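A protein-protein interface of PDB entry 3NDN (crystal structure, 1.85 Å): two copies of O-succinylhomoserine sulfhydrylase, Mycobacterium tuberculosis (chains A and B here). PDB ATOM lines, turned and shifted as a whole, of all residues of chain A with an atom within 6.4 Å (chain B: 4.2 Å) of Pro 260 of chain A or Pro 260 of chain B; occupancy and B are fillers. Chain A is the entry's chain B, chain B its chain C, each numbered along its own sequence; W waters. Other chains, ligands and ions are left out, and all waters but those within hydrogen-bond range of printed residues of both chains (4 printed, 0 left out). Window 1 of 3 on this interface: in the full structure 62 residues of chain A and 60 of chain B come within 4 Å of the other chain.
Ala 103 of chain A touches Ala 261 of chain B, and with the chains exchanged Ala 261 of chain A touches Ala 103 of chain B.
Ala 107 of chain A touches Gly 259 of chain B, and with the chains exchanged Gly 259 of chain A touches Ala 107 of chain B.
Gly 259 of chain A touches Ala 103 of chain B, but with the chains exchanged Ala 103 of chain A does not touch Gly 259 of chain B (4.005 Å).
Pro 260 of chain A touches its own counterpart, Pro 260 of chain B.
Pro 260 of chain A touches just one residue of chain B: Pro 260 (3.9 Å).
Printed residues of chain A within 4 Å of Pro 260 of chain B: Pro 260.
Of the printed residues of chain A, Thr 258 of chain B touches Ala 107 (3.2 Å).
Of the printed residues of chain A, Ala 103 of chain B touches Gly 259 (3.9 Å) and Ala 261 (3.8 Å).
Of the printed residues of chain B, Ala 107 of chain A touches Thr 258 and Gly 259.
Ala 101 of chain A touches none of the printed residues of chain B.
Water W2 bridges the backbone carbonyl oxygen (O) of Ala 103 of chain B and the backbone carbonyl oxygen (O) of Ala 261 of chain A.
Water W3 bridges the backbone carbonyl oxygen (O) of Thr 258 of chain A and the side-chain hydroxyl (OG1) of Thr 111 of chain B.
Water W4 bridges the backbone carbonyl oxygen of Ala 103 of chain A and the backbone carbonyl oxygen of Ala 261 of chain B.
Water W1 lies within hydrogen-bond range of O of Ala 261 of chain A (3.0 Å) and O of Ala 261 of chain B (3.0 Å).
The side-chain hydroxyl (OG) of Ser 104 of chain A lies within hydrogen-bond range of the backbone NH (N) of Ala 107 of chain A, at 3.1 Å.
The side-chain hydroxyl (OG1) of Thr 102 of chain A is in hydrogen-bond range of the backbone carbonyl oxygen (O) of Ser 104 of chain A.
The backbone carbonyl oxygen (O) of Leu 254 of chain A is in hydrogen-bond range of the side-chain hydroxyl (OG1) of Thr 258 of chain A (2.7 Å).
The backbone NH of Ala 103 of chain B is in hydrogen-bond range of the backbone carbonyl oxygen of Pro 260 of chain B (2.9 Å).
The backbone NH (N) of Ala 103 of chain A is in hydrogen-bond range of the backbone carbonyl oxygen (O) of Pro 260 of chain A.
The side-chain hydroxyl of Thr 111 of chain B sits at hydrogen-bond distance from the backbone carbonyl oxygen of Ala 107 of chain B.
Of the 10 printed residues of chain B, 6 touch a printed residue of chain A.
Among the printed residues, merely in contact across the chains: Ala 103 of chain A with Ala 261 of chain B (3.7 Å), Ala 107 of chain A with Gly 259 of chain B (3.5 Å), Gly 259 of chain A with Ala 103 of chain B (3.9 Å), Gly 259 of chain A with Ala 107 of chain B (3.6 Å), Pro 260 of chain A with Pro 260 of chain B (3.9 Å) and Ala 261 of chain A with Ala 103 of chain B (3.8 Å).
The side-chain hydroxyl of Ser 104 of chain A lies within hydrogen-bond range of the backbone carbonyl oxygen of Gly 259 of chain B (2.8 Å).
The backbone carbonyl oxygen (O) of Thr 258 of chain B sits close to the backbone NH (N) of Ala 107 of chain A (3.4 Å).
The backbone NH (N) of Ala 107 of chain B sits close to the backbone carbonyl oxygen (O) of Thr 258 of chain A (3.4 Å).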
ATOM      1  N   ARG A  77      -5.110  27.121 -22.527  1.00  0.00           N
ATOM      2  CA  ARG A  77      -3.922  27.129 -21.641  1.00  0.00           C
ATOM      3  C   ARG A  77      -3.513  25.721 -21.239  1.00  0.00           C
ATOM      4  O   ARG A  77      -2.328  25.452 -20.982  1.00  0.00           O
ATOM      5  CB  ARG A  77      -4.121  28.005 -20.388  1.00  0.00           C
ATOM      6  CG  ARG A  77      -2.799  28.597 -19.817  1.00  0.00           C
ATOM      7  CD  ARG A  77      -2.913  29.174 -18.383  1.00  0.00           C
ATOM      8  NE  ARG A  77      -3.964  30.183 -18.234  1.00  0.00           N
ATOM      9  CZ  ARG A  77      -5.140  29.969 -17.634  1.00  0.00           C
ATOM     10  NH1 ARG A  77      -6.030  30.948 -17.551  1.00  0.00           N
ATOM     11  NH2 ARG A  77      -5.443  28.773 -17.130  1.00  0.00           N
ATOM     12  N   ALA A 101       2.315  18.895 -23.845  1.00  0.00           N
ATOM     13  CA  ALA A 101       3.105  19.890 -24.625  1.00  0.00           C
ATOM     14  C   ALA A 101       3.393  21.197 -23.868  1.00  0.00           C
ATOM     15  O   ALA A 101       2.567  21.653 -23.054  1.00  0.00           O
ATOM     16  CB  ALA A 101       2.393  20.205 -25.970  1.00  0.00           C
ATOM     17  N   THR A 102       4.560  21.795 -24.129  1.00  0.00           N
ATOM     18  CA  THR A 102       4.981  23.061 -23.462  1.00  0.00           C
ATOM     19  C   THR A 102       5.516  24.149 -24.421  1.00  0.00           C
ATOM     20  O   THR A 102       5.837  23.857 -25.576  1.00  0.00           O
ATOM     21  CB  THR A 102       6.116  22.794 -22.411  1.00  0.00           C
ATOM     22  OG1 THR A 102       7.283  22.324 -23.091  1.00  0.00           O
ATOM     23  CG2 THR A 102       5.709  21.778 -21.361  1.00  0.00           C
ATOM     24  N   ALA A 103       5.663  25.395 -23.924  1.00  0.00           N
ATOM     25  CA  ALA A 103       6.169  26.523 -24.724  1.00  0.00           C
ATOM     26  C   ALA A 103       7.621  26.409 -25.242  1.00  0.00           C
ATOM     27  O   ALA A 103       7.957  26.986 -26.285  1.00  0.00           O
ATOM     28  CB  ALA A 103       5.978  27.863 -23.946  1.00  0.00           C
ATOM     29  N   SER A 104       8.466  25.681 -24.513  1.00  0.00           N
ATOM     30  CA  SER A 104       9.876  25.448 -24.897  1.00  0.00           C
ATOM     31  C   SER A 104      10.443  24.180 -24.241  1.00  0.00           C
ATOM     32  O   SER A 104       9.835  23.618 -23.304  1.00  0.00           O
ATOM     33  CB  SER A 104      10.749  26.649 -24.482  1.00  0.00           C
ATOM     34  OG  SER A 104      10.955  26.638 -23.058  1.00  0.00           O
ATOM     35  N   ALA A 107      10.953  24.888 -20.549  1.00  0.00           N
ATOM     36  CA  ALA A 107       9.688  24.784 -19.805  1.00  0.00           C
ATOM     37  C   ALA A 107       9.371  23.313 -19.477  1.00  0.00           C
ATOM     38  O   ALA A 107       8.843  23.012 -18.389  1.00  0.00           O
ATOM     39  CB  ALA A 107       8.534  25.408 -20.611  1.00  0.00           C
ATOM     40  N   THR A 111       9.340  22.322 -15.421  1.00  0.00           N
ATOM     41  CA  THR A 111       8.035  21.861 -14.944  1.00  0.00           C
ATOM     42  C   THR A 111       8.037  20.370 -14.554  1.00  0.00           C
ATOM     43  O   THR A 111       7.440  19.994 -13.531  1.00  0.00           O
ATOM     44  CB  THR A 111       6.904  22.168 -15.978  1.00  0.00           C
ATOM     45  OG1 THR A 111       6.857  23.580 -16.218  1.00  0.00           O
ATOM     46  CG2 THR A 111       5.554  21.713 -15.464  1.00  0.00           C
ATOM     47  N   LEU A 254       0.650  22.363 -12.451  1.00  0.00           N
ATOM     48  CA  LEU A 254       1.572  23.451 -12.803  1.00  0.00           C
ATOM     49  C   LEU A 254       1.267  24.037 -14.191  1.00  0.00           C
ATOM     50  O   LEU A 254       1.320  25.249 -14.382  1.00  0.00           O
ATOM     51  CB  LEU A 254       3.028  22.983 -12.725  1.00  0.00           C
ATOM     52  CG  LEU A 254       3.550  22.616 -11.334  1.00  0.00           C
ATOM     53  CD1 LEU A 254       4.877  21.877 -11.451  1.00  0.00           C
ATOM     54  CD2 LEU A 254       3.691  23.868 -10.455  1.00  0.00           C
ATOM     55  N   MET A 255       0.920  23.171 -15.140  1.00  0.00           N
ATOM     56  CA  MET A 255       0.610  23.613 -16.513  1.00  0.00           C
ATOM     57  C   MET A 255      -0.633  24.514 -16.545  1.00  0.00           C
ATOM     58  O   MET A 255      -0.592  25.604 -17.122  1.00  0.00           O
ATOM     59  CB  MET A 255       0.467  22.423 -17.484  1.00  0.00           C
ATOM     60  CG  MET A 255       1.781  21.710 -17.830  1.00  0.00           C
ATOM     61  SD  MET A 255       3.158  22.711 -18.470  1.00  0.00           S
ATOM     62  CE  MET A 255       2.533  23.300 -20.060  1.00  0.00           C
ATOM     63  N   ARG A 256      -1.702  24.084 -15.872  1.00  0.00           N
ATOM     64  CA  ARG A 256      -2.936  24.868 -15.781  1.00  0.00           C
ATOM     65  C   ARG A 256      -2.721  26.243 -15.133  1.00  0.00           C
ATOM     66  O   ARG A 256      -3.207  27.246 -15.654  1.00  0.00           O
ATOM     67  CB  ARG A 256      -4.016  24.110 -15.001  1.00  0.00           C
ATOM     68  CG  ARG A 256      -4.556  22.871 -15.695  1.00  0.00           C
ATOM     69  CD  ARG A 256      -5.962  22.517 -15.201  1.00  0.00           C
ATOM     70  NE  ARG A 256      -6.564  21.431 -15.983  1.00  0.00           N
ATOM     71  CZ  ARG A 256      -7.741  20.867 -15.710  1.00  0.00           C
ATOM     72  NH1 ARG A 256      -8.456  21.271 -14.668  1.00  0.00           N
ATOM     73  NH2 ARG A 256      -8.204  19.894 -16.481  1.00  0.00           N
ATOM     74  N   HIS A 257      -2.001  26.281 -14.004  1.00  0.00           N
ATOM     75  CA  HIS A 257      -1.933  27.499 -13.173  1.00  0.00           C
ATOM     76  C   HIS A 257      -0.685  28.392 -13.317  1.00  0.00           C
ATOM     77  O   HIS A 257      -0.757  29.598 -12.996  1.00  0.00           O
ATOM     78  CB  HIS A 257      -2.240  27.172 -11.688  1.00  0.00           C
ATOM     79  CG  HIS A 257      -3.476  26.347 -11.499  1.00  0.00           C
ATOM     80  ND1 HIS A 257      -4.744  26.836 -11.745  1.00  0.00           N
ATOM     81  CD2 HIS A 257      -3.639  25.058 -11.111  1.00  0.00           C
ATOM     82  CE1 HIS A 257      -5.633  25.882 -11.521  1.00  0.00           C
ATOM     83  NE2 HIS A 257      -4.989  24.793 -11.136  1.00  0.00           N
ATOM     84  N   THR A 258       0.441  27.839 -13.790  1.00  0.00           N
ATOM     85  CA  THR A 258       1.628  28.675 -14.125  1.00  0.00           C
ATOM     86  C   THR A 258       1.763  29.018 -15.638  1.00  0.00           C
ATOM     87  O   THR A 258       2.527  29.917 -16.018  1.00  0.00           O
ATOM     88  CB  THR A 258       2.976  28.099 -13.585  1.00  0.00           C
ATOM     89  OG1 THR A 258       3.389  26.972 -14.375  1.00  0.00           O
ATOM     90  CG2 THR A 258       2.845  27.682 -12.098  1.00  0.00           C
ATOM     91  N   GLY A 259       1.031  28.296 -16.479  1.00  0.00           N
ATOM     92  CA  GLY A 259       0.818  28.673 -17.891  1.00  0.00           C
ATOM     93  C   GLY A 259       1.939  28.765 -18.932  1.00  0.00           C
ATOM     94  O   GLY A 259       1.861  29.623 -19.812  1.00  0.00           O
ATOM     95  N   PRO A 260       2.956  27.866 -18.893  1.00  0.00           N
ATOM     96  CA  PRO A 260       3.932  27.878 -19.998  1.00  0.00           C
ATOM     97  C   PRO A 260       3.417  27.097 -21.235  1.00  0.00           C
ATOM     98  O   PRO A 260       3.964  26.056 -21.607  1.00  0.00           O
ATOM     99  CB  PRO A 260       5.179  27.231 -19.372  1.00  0.00           C
ATOM    100  CG  PRO A 260       4.644  26.313 -18.311  1.00  0.00           C
ATOM    101  CD  PRO A 260       3.263  26.822 -17.896  1.00  0.00           C
ATOM    102  N   ALA A 261       2.360  27.620 -21.850  1.00  0.00           N
ATOM    103  CA  ALA A 261       1.541  26.894 -22.815  1.00  0.00           C
ATOM    104  C   ALA A 261       2.100  26.956 -24.238  1.00  0.00           C
ATOM    105  O   ALA A 261       2.581  28.003 -24.655  1.00  0.00           O
ATOM    106  CB  ALA A 261       0.108  27.453 -22.800  1.00  0.00           C
ATOM    107  N   MET A 262       2.042  25.834 -24.967  1.00  0.00           N
ATOM    108  CA  MET A 262       2.355  25.818 -26.421  1.00  0.00           C
ATOM    109  C   MET A 262       1.246  26.506 -27.233  1.00  0.00           C
ATOM    110  O   MET A 262       0.061  26.246 -27.012  1.00  0.00           O
ATOM    111  CB  MET A 262       2.524  24.359 -26.931  1.00  0.00           C
ATOM    112  CG  MET A 262       2.903  24.234 -28.455  1.00  0.00           C
ATOM    113  SD  MET A 262       3.167  22.535 -29.037  1.00  0.00           S
ATOM    114  CE  MET A 262       4.777  22.166 -28.346  1.00  0.00           C
ATOM    115  N   THR B 102       5.350  37.083 -22.377  1.00  0.00           N
ATOM    116  CA  THR B 102       5.239  35.709 -21.845  1.00  0.00           C
ATOM    117  C   THR B 102       4.237  34.832 -22.627  1.00  0.00           C
ATOM    118  O   THR B 102       3.442  35.346 -23.414  1.00  0.00           O
ATOM    119  CB  THR B 102       4.808  35.723 -20.336  1.00  0.00           C
ATOM    120  OG1 THR B 102       3.446  36.146 -20.244  1.00  0.00           O
ATOM    121  CG2 THR B 102       5.700  36.647 -19.485  1.00  0.00           C
ATOM    122  N   ALA B 103       4.248  33.518 -22.388  1.00  0.00           N
ATOM    123  CA  ALA B 103       3.356  32.576 -23.087  1.00  0.00           C
ATOM    124  C   ALA B 103       1.844  32.705 -22.792  1.00  0.00           C
ATOM    125  O   ALA B 103       1.011  32.312 -23.633  1.00  0.00           O
ATOM    126  CB  ALA B 103       3.825  31.132 -22.874  1.00  0.00           C
ATOM    127  N   ALA B 107       1.368  32.962 -16.874  1.00  0.00           N
ATOM    128  CA  ALA B 107       2.830  32.876 -16.831  1.00  0.00           C
ATOM    129  C   ALA B 107       3.418  34.228 -16.382  1.00  0.00           C
ATOM    130  O   ALA B 107       4.457  34.272 -15.713  1.00  0.00           O
ATOM    131  CB  ALA B 107       3.413  32.459 -18.206  1.00  0.00           C
ATOM    132  N   THR B 111       5.489  34.323 -12.862  1.00  0.00           N
ATOM    133  CA  THR B 111       6.888  34.700 -13.037  1.00  0.00           C
ATOM    134  C   THR B 111       7.216  36.055 -12.372  1.00  0.00           C
ATOM    135  O   THR B 111       8.301  36.224 -11.807  1.00  0.00           O
ATOM    136  CB  THR B 111       7.301  34.650 -14.538  1.00  0.00           C
ATOM    137  OG1 THR B 111       7.177  33.289 -15.005  1.00  0.00           O
ATOM    138  CG2 THR B 111       8.740  35.097 -14.731  1.00  0.00           C
ATOM    139  N   MET B 255      12.958  33.990 -17.042  1.00  0.00           N
ATOM    140  CA  MET B 255      12.491  33.850 -18.434  1.00  0.00           C
ATOM    141  C   MET B 255      13.445  33.031 -19.302  1.00  0.00           C
ATOM    142  O   MET B 255      12.996  32.112 -19.991  1.00  0.00           O
ATOM    143  CB  MET B 255      12.179  35.200 -19.086  1.00  0.00           C
ATOM    144  CG  MET B 255      10.931  35.923 -18.534  1.00  0.00           C
ATOM    145  SD  MET B 255       9.319  35.074 -18.616  1.00  0.00           S
ATOM    146  CE  MET B 255       9.166  34.827 -20.409  1.00  0.00           C
ATOM    147  N   THR B 258      13.738  29.154 -17.254  1.00  0.00           N
ATOM    148  CA  THR B 258      12.524  28.319 -17.162  1.00  0.00           C
ATOM    149  C   THR B 258      11.621  28.355 -18.420  1.00  0.00           C
ATOM    150  O   THR B 258      10.684  27.574 -18.524  1.00  0.00           O
ATOM    151  CB  THR B 258      11.654  28.615 -15.904  1.00  0.00           C
ATOM    152  OG1 THR B 258      10.950  29.858 -16.051  1.00  0.00           O
ATOM    153  CG2 THR B 258      12.505  28.636 -14.625  1.00  0.00           C
ATOM    154  N   GLY B 259      11.888  29.283 -19.333  1.00  0.00           N
ATOM    155  CA  GLY B 259      11.295  29.251 -20.690  1.00  0.00           C
ATOM    156  C   GLY B 259       9.788  29.335 -20.955  1.00  0.00           C
ATOM    157  O   GLY B 259       9.302  28.608 -21.840  1.00  0.00           O
ATOM    158  N   PRO B 260       9.029  30.208 -20.236  1.00  0.00           N
ATOM    159  CA  PRO B 260       7.616  30.367 -20.657  1.00  0.00           C
ATOM    160  C   PRO B 260       7.439  31.422 -21.784  1.00  0.00           C
ATOM    161  O   PRO B 260       6.794  32.488 -21.592  1.00  0.00           O
ATOM    162  CB  PRO B 260       6.900  30.763 -19.355  1.00  0.00           C
ATOM    163  CG  PRO B 260       7.936  31.470 -18.547  1.00  0.00           C
ATOM    164  CD  PRO B 260       9.319  30.979 -19.004  1.00  0.00           C
ATOM    165  N   ALA B 261       8.030  31.102 -22.941  1.00  0.00           N
ATOM    166  CA  ALA B 261       8.265  32.048 -24.047  1.00  0.00           C
ATOM    167  C   ALA B 261       7.048  32.282 -24.956  1.00  0.00           C
ATOM    168  O   ALA B 261       6.355  31.328 -25.327  1.00  0.00           O
ATOM    169  CB  ALA B 261       9.463  31.581 -24.900  1.00  0.00           C
ATOM    170  N   MET B 262       6.820  33.550 -25.313  1.00  0.00           N
ATOM    171  CA  MET B 262       5.836  33.943 -26.339  1.00  0.00           C
ATOM    172  C   MET B 262       6.367  33.562 -27.725  1.00  0.00           C
ATOM    173  O   MET B 262       7.551  33.779 -28.037  1.00  0.00           O
ATOM    174  CB  MET B 262       5.523  35.466 -26.283  1.00  0.00           C
ATOM    175  CG  MET B 262       4.396  35.923 -27.299  1.00  0.00           C
ATOM    176  SD  MET B 262       4.064  37.697 -27.256  1.00  0.00           S
ATOM    177  CE  MET B 262       3.015  37.754 -25.795  1.00  0.00           C
HETATM  178  O   HOH W   1       3.997  29.840 -26.512  1.00  0.00           O
HETATM  179  O   HOH W   2       0.830  30.371 -25.732  1.00  0.00           O
HETATM  180  O   HOH W   3       5.330  30.688 -15.979  1.00  0.00           O
HETATM  181  O   HOH W   4       7.239  29.515 -27.620  1.00  0.00           O
